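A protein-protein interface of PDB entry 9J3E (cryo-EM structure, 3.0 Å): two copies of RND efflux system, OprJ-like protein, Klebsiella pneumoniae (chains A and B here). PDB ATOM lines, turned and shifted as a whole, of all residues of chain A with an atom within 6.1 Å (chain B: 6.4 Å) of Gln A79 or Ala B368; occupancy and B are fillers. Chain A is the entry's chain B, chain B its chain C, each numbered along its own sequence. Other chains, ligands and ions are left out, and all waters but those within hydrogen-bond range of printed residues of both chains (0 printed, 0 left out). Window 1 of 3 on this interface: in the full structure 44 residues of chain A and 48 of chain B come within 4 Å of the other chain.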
ATOM      1  N   ASN A  74      -2.560  21.753 -28.147  1.00  0.00           N
ATOM      2  CA  ASN A  74      -1.201  21.386 -27.771  1.00  0.00           C
ATOM      3  C   ASN A  74      -1.074  19.875 -27.660  1.00  0.00           C
ATOM      4  O   ASN A  74      -1.910  19.207 -27.049  1.00  0.00           O
ATOM      5  CB  ASN A  74      -0.810  22.042 -26.449  1.00  0.00           C
ATOM      6  CG  ASN A  74       0.621  21.752 -26.062  1.00  0.00           C
ATOM      7  OD1 ASN A  74       0.906  20.758 -25.396  1.00  0.00           O
ATOM      8  ND2 ASN A  74       1.533  22.622 -26.474  1.00  0.00           N
ATOM      9  N   ARG A  75      -0.011  19.337 -28.252  1.00  0.00           N
ATOM     10  CA  ARG A  75       0.172  17.893 -28.293  1.00  0.00           C
ATOM     11  C   ARG A  75       0.585  17.317 -26.947  1.00  0.00           C
ATOM     12  O   ARG A  75       0.106  16.246 -26.568  1.00  0.00           O
ATOM     13  CB  ARG A  75       1.201  17.522 -29.359  1.00  0.00           C
ATOM     14  CG  ARG A  75       0.831  17.990 -30.749  1.00  0.00           C
ATOM     15  CD  ARG A  75      -0.615  17.656 -31.052  1.00  0.00           C
ATOM     16  NE  ARG A  75      -0.946  17.845 -32.457  1.00  0.00           N
ATOM     17  CZ  ARG A  75      -2.001  18.518 -32.892  1.00  0.00           C
ATOM     18  NH1 ARG A  75      -2.862  19.071 -32.054  1.00  0.00           N
ATOM     19  NH2 ARG A  75      -2.201  18.638 -34.202  1.00  0.00           N
ATOM     20  N   SER A  76       1.467  17.995 -26.214  1.00  0.00           N
ATOM     21  CA  SER A  76       1.833  17.511 -24.888  1.00  0.00           C
ATOM     22  C   SER A  76       0.656  17.581 -23.927  1.00  0.00           C
ATOM     23  O   SER A  76       0.500  16.710 -23.066  1.00  0.00           O
ATOM     24  CB  SER A  76       3.011  18.312 -24.344  1.00  0.00           C
ATOM     25  OG  SER A  76       4.033  18.426 -25.316  1.00  0.00           O
ATOM     26  N   LEU A  77      -0.180  18.606 -24.052  1.00  0.00           N
ATOM     27  CA  LEU A  77      -1.370  18.689 -23.219  1.00  0.00           C
ATOM     28  C   LEU A  77      -2.326  17.537 -23.518  1.00  0.00           C
ATOM     29  O   LEU A  77      -2.859  16.900 -22.595  1.00  0.00           O
ATOM     30  CB  LEU A  77      -2.023  20.055 -23.439  1.00  0.00           C
ATOM     31  CG  LEU A  77      -3.091  20.622 -22.511  1.00  0.00           C
ATOM     32  CD1 LEU A  77      -4.471  20.181 -22.943  1.00  0.00           C
ATOM     33  CD2 LEU A  77      -2.802  20.206 -21.080  1.00  0.00           C
ATOM     34  N   ARG A  78      -2.528  17.235 -24.803  1.00  0.00           N
ATOM     35  CA  ARG A  78      -3.331  16.075 -25.171  1.00  0.00           C
ATOM     36  C   ARG A  78      -2.706  14.798 -24.631  1.00  0.00           C
ATOM     37  O   ARG A  78      -3.415  13.878 -24.212  1.00  0.00           O
ATOM     38  CB  ARG A  78      -3.486  16.000 -26.688  1.00  0.00           C
ATOM     39  CG  ARG A  78      -4.520  16.962 -27.252  1.00  0.00           C
ATOM     40  CD  ARG A  78      -4.491  17.039 -28.776  1.00  0.00           C
ATOM     41  NE  ARG A  78      -4.666  15.742 -29.419  1.00  0.00           N
ATOM     42  CZ  ARG A  78      -3.677  14.966 -29.843  1.00  0.00           C
ATOM     43  NH1 ARG A  78      -2.412  15.321 -29.704  1.00  0.00           N
ATOM     44  NH2 ARG A  78      -3.967  13.805 -30.423  1.00  0.00           N
ATOM     45  N   GLN A  79      -1.375  14.731 -24.625  1.00  0.00           N
ATOM     46  CA  GLN A  79      -0.681  13.606 -24.012  1.00  0.00           C
ATOM     47  C   GLN A  79      -1.015  13.503 -22.532  1.00  0.00           C
ATOM     48  O   GLN A  79      -1.143  12.405 -21.987  1.00  0.00           O
ATOM     49  CB  GLN A  79       0.825  13.764 -24.206  1.00  0.00           C
ATOM     50  CG  GLN A  79       1.609  12.477 -24.153  1.00  0.00           C
ATOM     51  CD  GLN A  79       2.377  12.231 -25.427  1.00  0.00           C
ATOM     52  OE1 GLN A  79       1.907  12.552 -26.514  1.00  0.00           O
ATOM     53  NE2 GLN A  79       3.571  11.669 -25.300  1.00  0.00           N
ATOM     54  N   ALA A  80      -1.140  14.644 -21.862  1.00  0.00           N
ATOM     55  CA  ALA A  80      -1.469  14.625 -20.440  1.00  0.00           C
ATOM     56  C   ALA A  80      -2.869  14.070 -20.196  1.00  0.00           C
ATOM     57  O   ALA A  80      -3.061  13.210 -19.325  1.00  0.00           O
ATOM     58  CB  ALA A  80      -1.339  16.029 -19.854  1.00  0.00           C
ATOM     59  N   LEU A  81      -3.863  14.549 -20.945  1.00  0.00           N
ATOM     60  CA  LEU A  81      -5.203  13.978 -20.778  1.00  0.00           C
ATOM     61  C   LEU A  81      -5.243  12.514 -21.200  1.00  0.00           C
ATOM     62  O   LEU A  81      -6.026  11.721 -20.664  1.00  0.00           O
ATOM     63  CB  LEU A  81      -6.268  14.776 -21.532  1.00  0.00           C
ATOM     64  CG  LEU A  81      -6.592  16.209 -21.105  1.00  0.00           C
ATOM     65  CD1 LEU A  81      -6.642  16.317 -19.586  1.00  0.00           C
ATOM     66  CD2 LEU A  81      -5.652  17.214 -21.677  1.00  0.00           C
ATOM     67  N   LEU A  82      -4.410  12.125 -22.151  1.00  0.00           N
ATOM     68  CA  LEU A  82      -4.372  10.714 -22.498  1.00  0.00           C
ATOM     69  C   LEU A  82      -3.726   9.898 -21.384  1.00  0.00           C
ATOM     70  O   LEU A  82      -4.126   8.758 -21.137  1.00  0.00           O
ATOM     71  CB  LEU A  82      -3.661  10.552 -23.836  1.00  0.00           C
ATOM     72  CG  LEU A  82      -4.633  10.457 -25.015  1.00  0.00           C
ATOM     73  CD1 LEU A  82      -5.764  11.462 -24.900  1.00  0.00           C
ATOM     74  CD2 LEU A  82      -3.878  10.755 -26.275  1.00  0.00           C
ATOM     75  N   ASP A  83      -2.766  10.481 -20.665  1.00  0.00           N
ATOM     76  CA  ASP A  83      -2.226   9.814 -19.487  1.00  0.00           C
ATOM     77  C   ASP A  83      -3.281   9.679 -18.402  1.00  0.00           C
ATOM     78  O   ASP A  83      -3.294   8.685 -17.676  1.00  0.00           O
ATOM     79  CB  ASP A  83      -1.015  10.568 -18.939  1.00  0.00           C
ATOM     80  CG  ASP A  83       0.184  10.502 -19.866  1.00  0.00           C
ATOM     81  OD1 ASP A  83       0.375   9.458 -20.519  1.00  0.00           O
ATOM     82  OD2 ASP A  83       0.941  11.494 -19.937  1.00  0.00           O
ATOM     83  N   ILE A  84      -4.153  10.679 -18.252  1.00  0.00           N
ATOM     84  CA  ILE A  84      -5.237  10.546 -17.275  1.00  0.00           C
ATOM     85  C   ILE A  84      -6.210   9.447 -17.678  1.00  0.00           C
ATOM     86  O   ILE A  84      -6.670   8.673 -16.832  1.00  0.00           O
ATOM     87  CB  ILE A  84      -5.945  11.887 -17.010  1.00  0.00           C
ATOM     88  CG1 ILE A  84      -6.591  11.807 -15.636  1.00  0.00           C
ATOM     89  CG2 ILE A  84      -7.055  12.176 -17.994  1.00  0.00           C
ATOM     90  CD1 ILE A  84      -5.639  11.701 -14.542  1.00  0.00           C
ATOM     91  N   GLU B 363      -6.124   1.179 -25.979  1.00  0.00           N
ATOM     92  CA  GLU B 363      -6.648   2.225 -26.852  1.00  0.00           C
ATOM     93  C   GLU B 363      -6.075   3.587 -26.491  1.00  0.00           C
ATOM     94  O   GLU B 363      -5.576   4.315 -27.361  1.00  0.00           O
ATOM     95  CB  GLU B 363      -8.175   2.250 -26.764  1.00  0.00           C
ATOM     96  CG  GLU B 363      -8.894   3.101 -27.812  1.00  0.00           C
ATOM     97  CD  GLU B 363      -8.780   2.581 -29.238  1.00  0.00           C
ATOM     98  OE1 GLU B 363      -7.998   1.643 -29.497  1.00  0.00           O
ATOM     99  OE2 GLU B 363      -9.491   3.119 -30.111  1.00  0.00           O
ATOM    100  N   VAL B 364      -6.129   3.947 -25.211  1.00  0.00           N
ATOM    101  CA  VAL B 364      -5.654   5.263 -24.813  1.00  0.00           C
ATOM    102  C   VAL B 364      -4.141   5.338 -24.947  1.00  0.00           C
ATOM    103  O   VAL B 364      -3.583   6.401 -25.228  1.00  0.00           O
ATOM    104  CB  VAL B 364      -6.120   5.602 -23.389  1.00  0.00           C
ATOM    105  CG1 VAL B 364      -5.604   4.591 -22.398  1.00  0.00           C
ATOM    106  CG2 VAL B 364      -5.669   6.979 -23.024  1.00  0.00           C
ATOM    107  N   ARG B 365      -3.451   4.214 -24.768  1.00  0.00           N
ATOM    108  CA  ARG B 365      -2.008   4.209 -24.957  1.00  0.00           C
ATOM    109  C   ARG B 365      -1.649   4.451 -26.416  1.00  0.00           C
ATOM    110  O   ARG B 365      -0.698   5.179 -26.718  1.00  0.00           O
ATOM    111  CB  ARG B 365      -1.426   2.888 -24.471  1.00  0.00           C
ATOM    112  CG  ARG B 365       0.071   2.893 -24.381  1.00  0.00           C
ATOM    113  CD  ARG B 365       0.528   3.435 -23.045  1.00  0.00           C
ATOM    114  NE  ARG B 365       0.376   2.455 -21.977  1.00  0.00           N
ATOM    115  CZ  ARG B 365       1.096   1.347 -21.865  1.00  0.00           C
ATOM    116  NH1 ARG B 365       2.045   1.046 -22.737  1.00  0.00           N
ATOM    117  NH2 ARG B 365       0.864   0.523 -20.848  1.00  0.00           N
ATOM    118  N   GLN B 366      -2.398   3.849 -27.339  1.00  0.00           N
ATOM    119  CA  GLN B 366      -2.157   4.110 -28.754  1.00  0.00           C
ATOM    120  C   GLN B 366      -2.478   5.556 -29.101  1.00  0.00           C
ATOM    121  O   GLN B 366      -1.777   6.182 -29.905  1.00  0.00           O
ATOM    122  CB  GLN B 366      -2.974   3.152 -29.616  1.00  0.00           C
ATOM    123  CG  GLN B 366      -3.073   3.569 -31.067  1.00  0.00           C
ATOM    124  CD  GLN B 366      -4.444   4.092 -31.425  1.00  0.00           C
ATOM    125  OE1 GLN B 366      -5.432   3.772 -30.768  1.00  0.00           O
ATOM    126  NE2 GLN B 366      -4.510   4.904 -32.471  1.00  0.00           N
ATOM    127  N   ASP B 367      -3.531   6.110 -28.499  1.00  0.00           N
ATOM    128  CA  ASP B 367      -3.813   7.528 -28.703  1.00  0.00           C
ATOM    129  C   ASP B 367      -2.671   8.392 -28.184  1.00  0.00           C
ATOM    130  O   ASP B 367      -2.307   9.399 -28.805  1.00  0.00           O
ATOM    131  CB  ASP B 367      -5.125   7.911 -28.022  1.00  0.00           C
ATOM    132  CG  ASP B 367      -6.303   7.120 -28.540  1.00  0.00           C
ATOM    133  OD1 ASP B 367      -6.220   6.609 -29.676  1.00  0.00           O
ATOM    134  OD2 ASP B 367      -7.316   7.016 -27.819  1.00  0.00           O
ATOM    135  N   ALA B 368      -2.104   8.026 -27.034  1.00  0.00           N
ATOM    136  CA  ALA B 368      -0.971   8.765 -26.492  1.00  0.00           C
ATOM    137  C   ALA B 368       0.235   8.655 -27.406  1.00  0.00           C
ATOM    138  O   ALA B 368       1.006   9.607 -27.545  1.00  0.00           O
ATOM    139  CB  ALA B 368      -0.631   8.260 -25.092  1.00  0.00           C
ATOM    140  N   ALA B 369       0.420   7.497 -28.032  1.00  0.00           N
ATOM    141  CA  ALA B 369       1.480   7.360 -29.024  1.00  0.00           C
ATOM    142  C   ALA B 369       1.229   8.271 -30.217  1.00  0.00           C
ATOM    143  O   ALA B 369       2.167   8.849 -30.773  1.00  0.00           O
ATOM    144  CB  ALA B 369       1.600   5.907 -29.473  1.00  0.00           C
ATOM    145  N   VAL B 370      -0.032   8.401 -30.633  1.00  0.00           N
ATOM    146  CA  VAL B 370      -0.365   9.327 -31.714  1.00  0.00           C
ATOM    147  C   VAL B 370       0.001  10.751 -31.323  1.00  0.00           C
ATOM    148  O   VAL B 370       0.618  11.496 -32.100  1.00  0.00           O
ATOM    149  CB  VAL B 370      -1.860   9.220 -32.067  1.00  0.00           C
ATOM    150  CG1 VAL B 370      -2.246  10.306 -33.051  1.00  0.00           C
ATOM    151  CG2 VAL B 370      -2.185   7.855 -32.623  1.00  0.00           C
ATOM    152  N   ALA B 371      -0.379  11.149 -30.111  1.00  0.00           N
ATOM    153  CA  ALA B 371      -0.074  12.495 -29.642  1.00  0.00           C
ATOM    154  C   ALA B 371       1.429  12.705 -29.535  1.00  0.00           C
ATOM    155  O   ALA B 371       1.932  13.788 -29.840  1.00  0.00           O
ATOM    156  CB  ALA B 371      -0.754  12.753 -28.300  1.00  0.00           C
ATOM    157  N   ASP B 372       2.158  11.683 -29.094  1.00  0.00           N
ATOM    158  CA  ASP B 372       3.610  11.774 -29.007  1.00  0.00           C
ATOM    159  C   ASP B 372       4.228  11.926 -30.387  1.00  0.00           C
ATOM    160  O   ASP B 372       5.176  12.693 -30.564  1.00  0.00           O
ATOM    161  CB  ASP B 372       4.158  10.535 -28.302  1.00  0.00           C
ATOM    162  CG  ASP B 372       5.661  10.570 -28.132  1.00  0.00           C
ATOM    163  OD1 ASP B 372       6.239   9.514 -27.800  1.00  0.00           O
ATOM    164  OD2 ASP B 372       6.265  11.648 -28.298  1.00  0.00           O
ATOM    165  N   TYR B 373       3.712  11.196 -31.370  1.00  0.00           N
ATOM    166  CA  TYR B 373       4.194  11.340 -32.737  1.00  0.00           C
ATOM    167  C   TYR B 373       3.994  12.765 -33.229  1.00  0.00           C
ATOM    168  O   TYR B 373       4.914  13.388 -33.778  1.00  0.00           O
ATOM    169  CB  TYR B 373       3.462  10.346 -33.636  1.00  0.00           C
ATOM    170  CG  TYR B 373       3.863  10.384 -35.087  1.00  0.00           C
ATOM    171  CD1 TYR B 373       2.993  10.865 -36.051  1.00  0.00           C
ATOM    172  CD2 TYR B 373       5.096   9.909 -35.498  1.00  0.00           C
ATOM    173  CE1 TYR B 373       3.349  10.890 -37.379  1.00  0.00           C
ATOM    174  CE2 TYR B 373       5.461   9.931 -36.824  1.00  0.00           C
ATOM    175  CZ  TYR B 373       4.584  10.424 -37.760  1.00  0.00           C
ATOM    176  OH  TYR B 373       4.945  10.446 -39.085  1.00  0.00           O
ATOM    177  N   GLY B 375       3.609  15.466 -31.390  1.00  0.00           N
ATOM    178  CA  GLY B 375       4.429  16.380 -30.618  1.00  0.00           C
ATOM    179  C   GLY B 375       5.885  16.343 -31.032  1.00  0.00           C
ATOM    180  O   GLY B 375       6.552  17.374 -31.075  1.00  0.00           O
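OE1 of Gln A79 lies close to O of Ala B368 (3.2 Å).
The side-chain amide oxygen (OE1) of Gln A79 sits at hydrogen-bond distance from the backbone NH (N) of Asp B372 (2.7 Å).
The side-chain carboxylate (OD1) of Asp B367 sits close to the side-chain amide oxygen (OE1) of Gln B366 (3.1 Å).
Ala B371 touches Arg A75.
Arg A75 touches Gly B375 (CB to CA, 3.6 Å).
Arg A78 touches Ala B371 (NH1 to CB, 3.4 Å).
Gln A79 touches Ala B371 (OE1 to C, 3.1 Å).
CG2 of Val B364 touches O of Leu A82, at 3.0 Å.
Leu A82 touches Asp B367.
Leu A82 touches Ala B368.
Printed residues of chain B within 4 Å of Arg A75: Ala B371 and Gly B375.
Of the printed residues of chain B, Gln A79 touches Ala B368 (3.2 Å), Ala B371 (3.1 Å) and Asp B372 (2.7 Å).
Printed residues of chain A within 4 Å of Val B364: Leu A82.
Of the printed residues of chain A, Asp B367 touches Leu A82 (3.3 Å).
Of the printed residues of chain A, Ala B368 touches Gln A79 and Leu A82.
Ala B369 touches none of the printed residues of chain A.
Of the printed residues of chain A, Ala B371 touches Arg A75 (3.8 Å), Arg A78 (3.4 Å) and Gln A79 (3.1 Å).
Tyr B373 touches none of the printed residues of chain A.
Printed residues of chain A within 4 Å of Gly B375: Arg A75.
The nearest printed residue of chain A that does not touch Asp B372 is Arg A75 (5.6 Å).
Hydrophobic or aromatic side chains of chain B that line the printed part of chain A: Val B364 and Ala B371.
Among the printed residues, 9 pairs touch across the chains.
No position is printed for both chains.
Of the 9 pairs that touch across the chains among the printed residues, none has its exchanged pair printed and touching as well.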
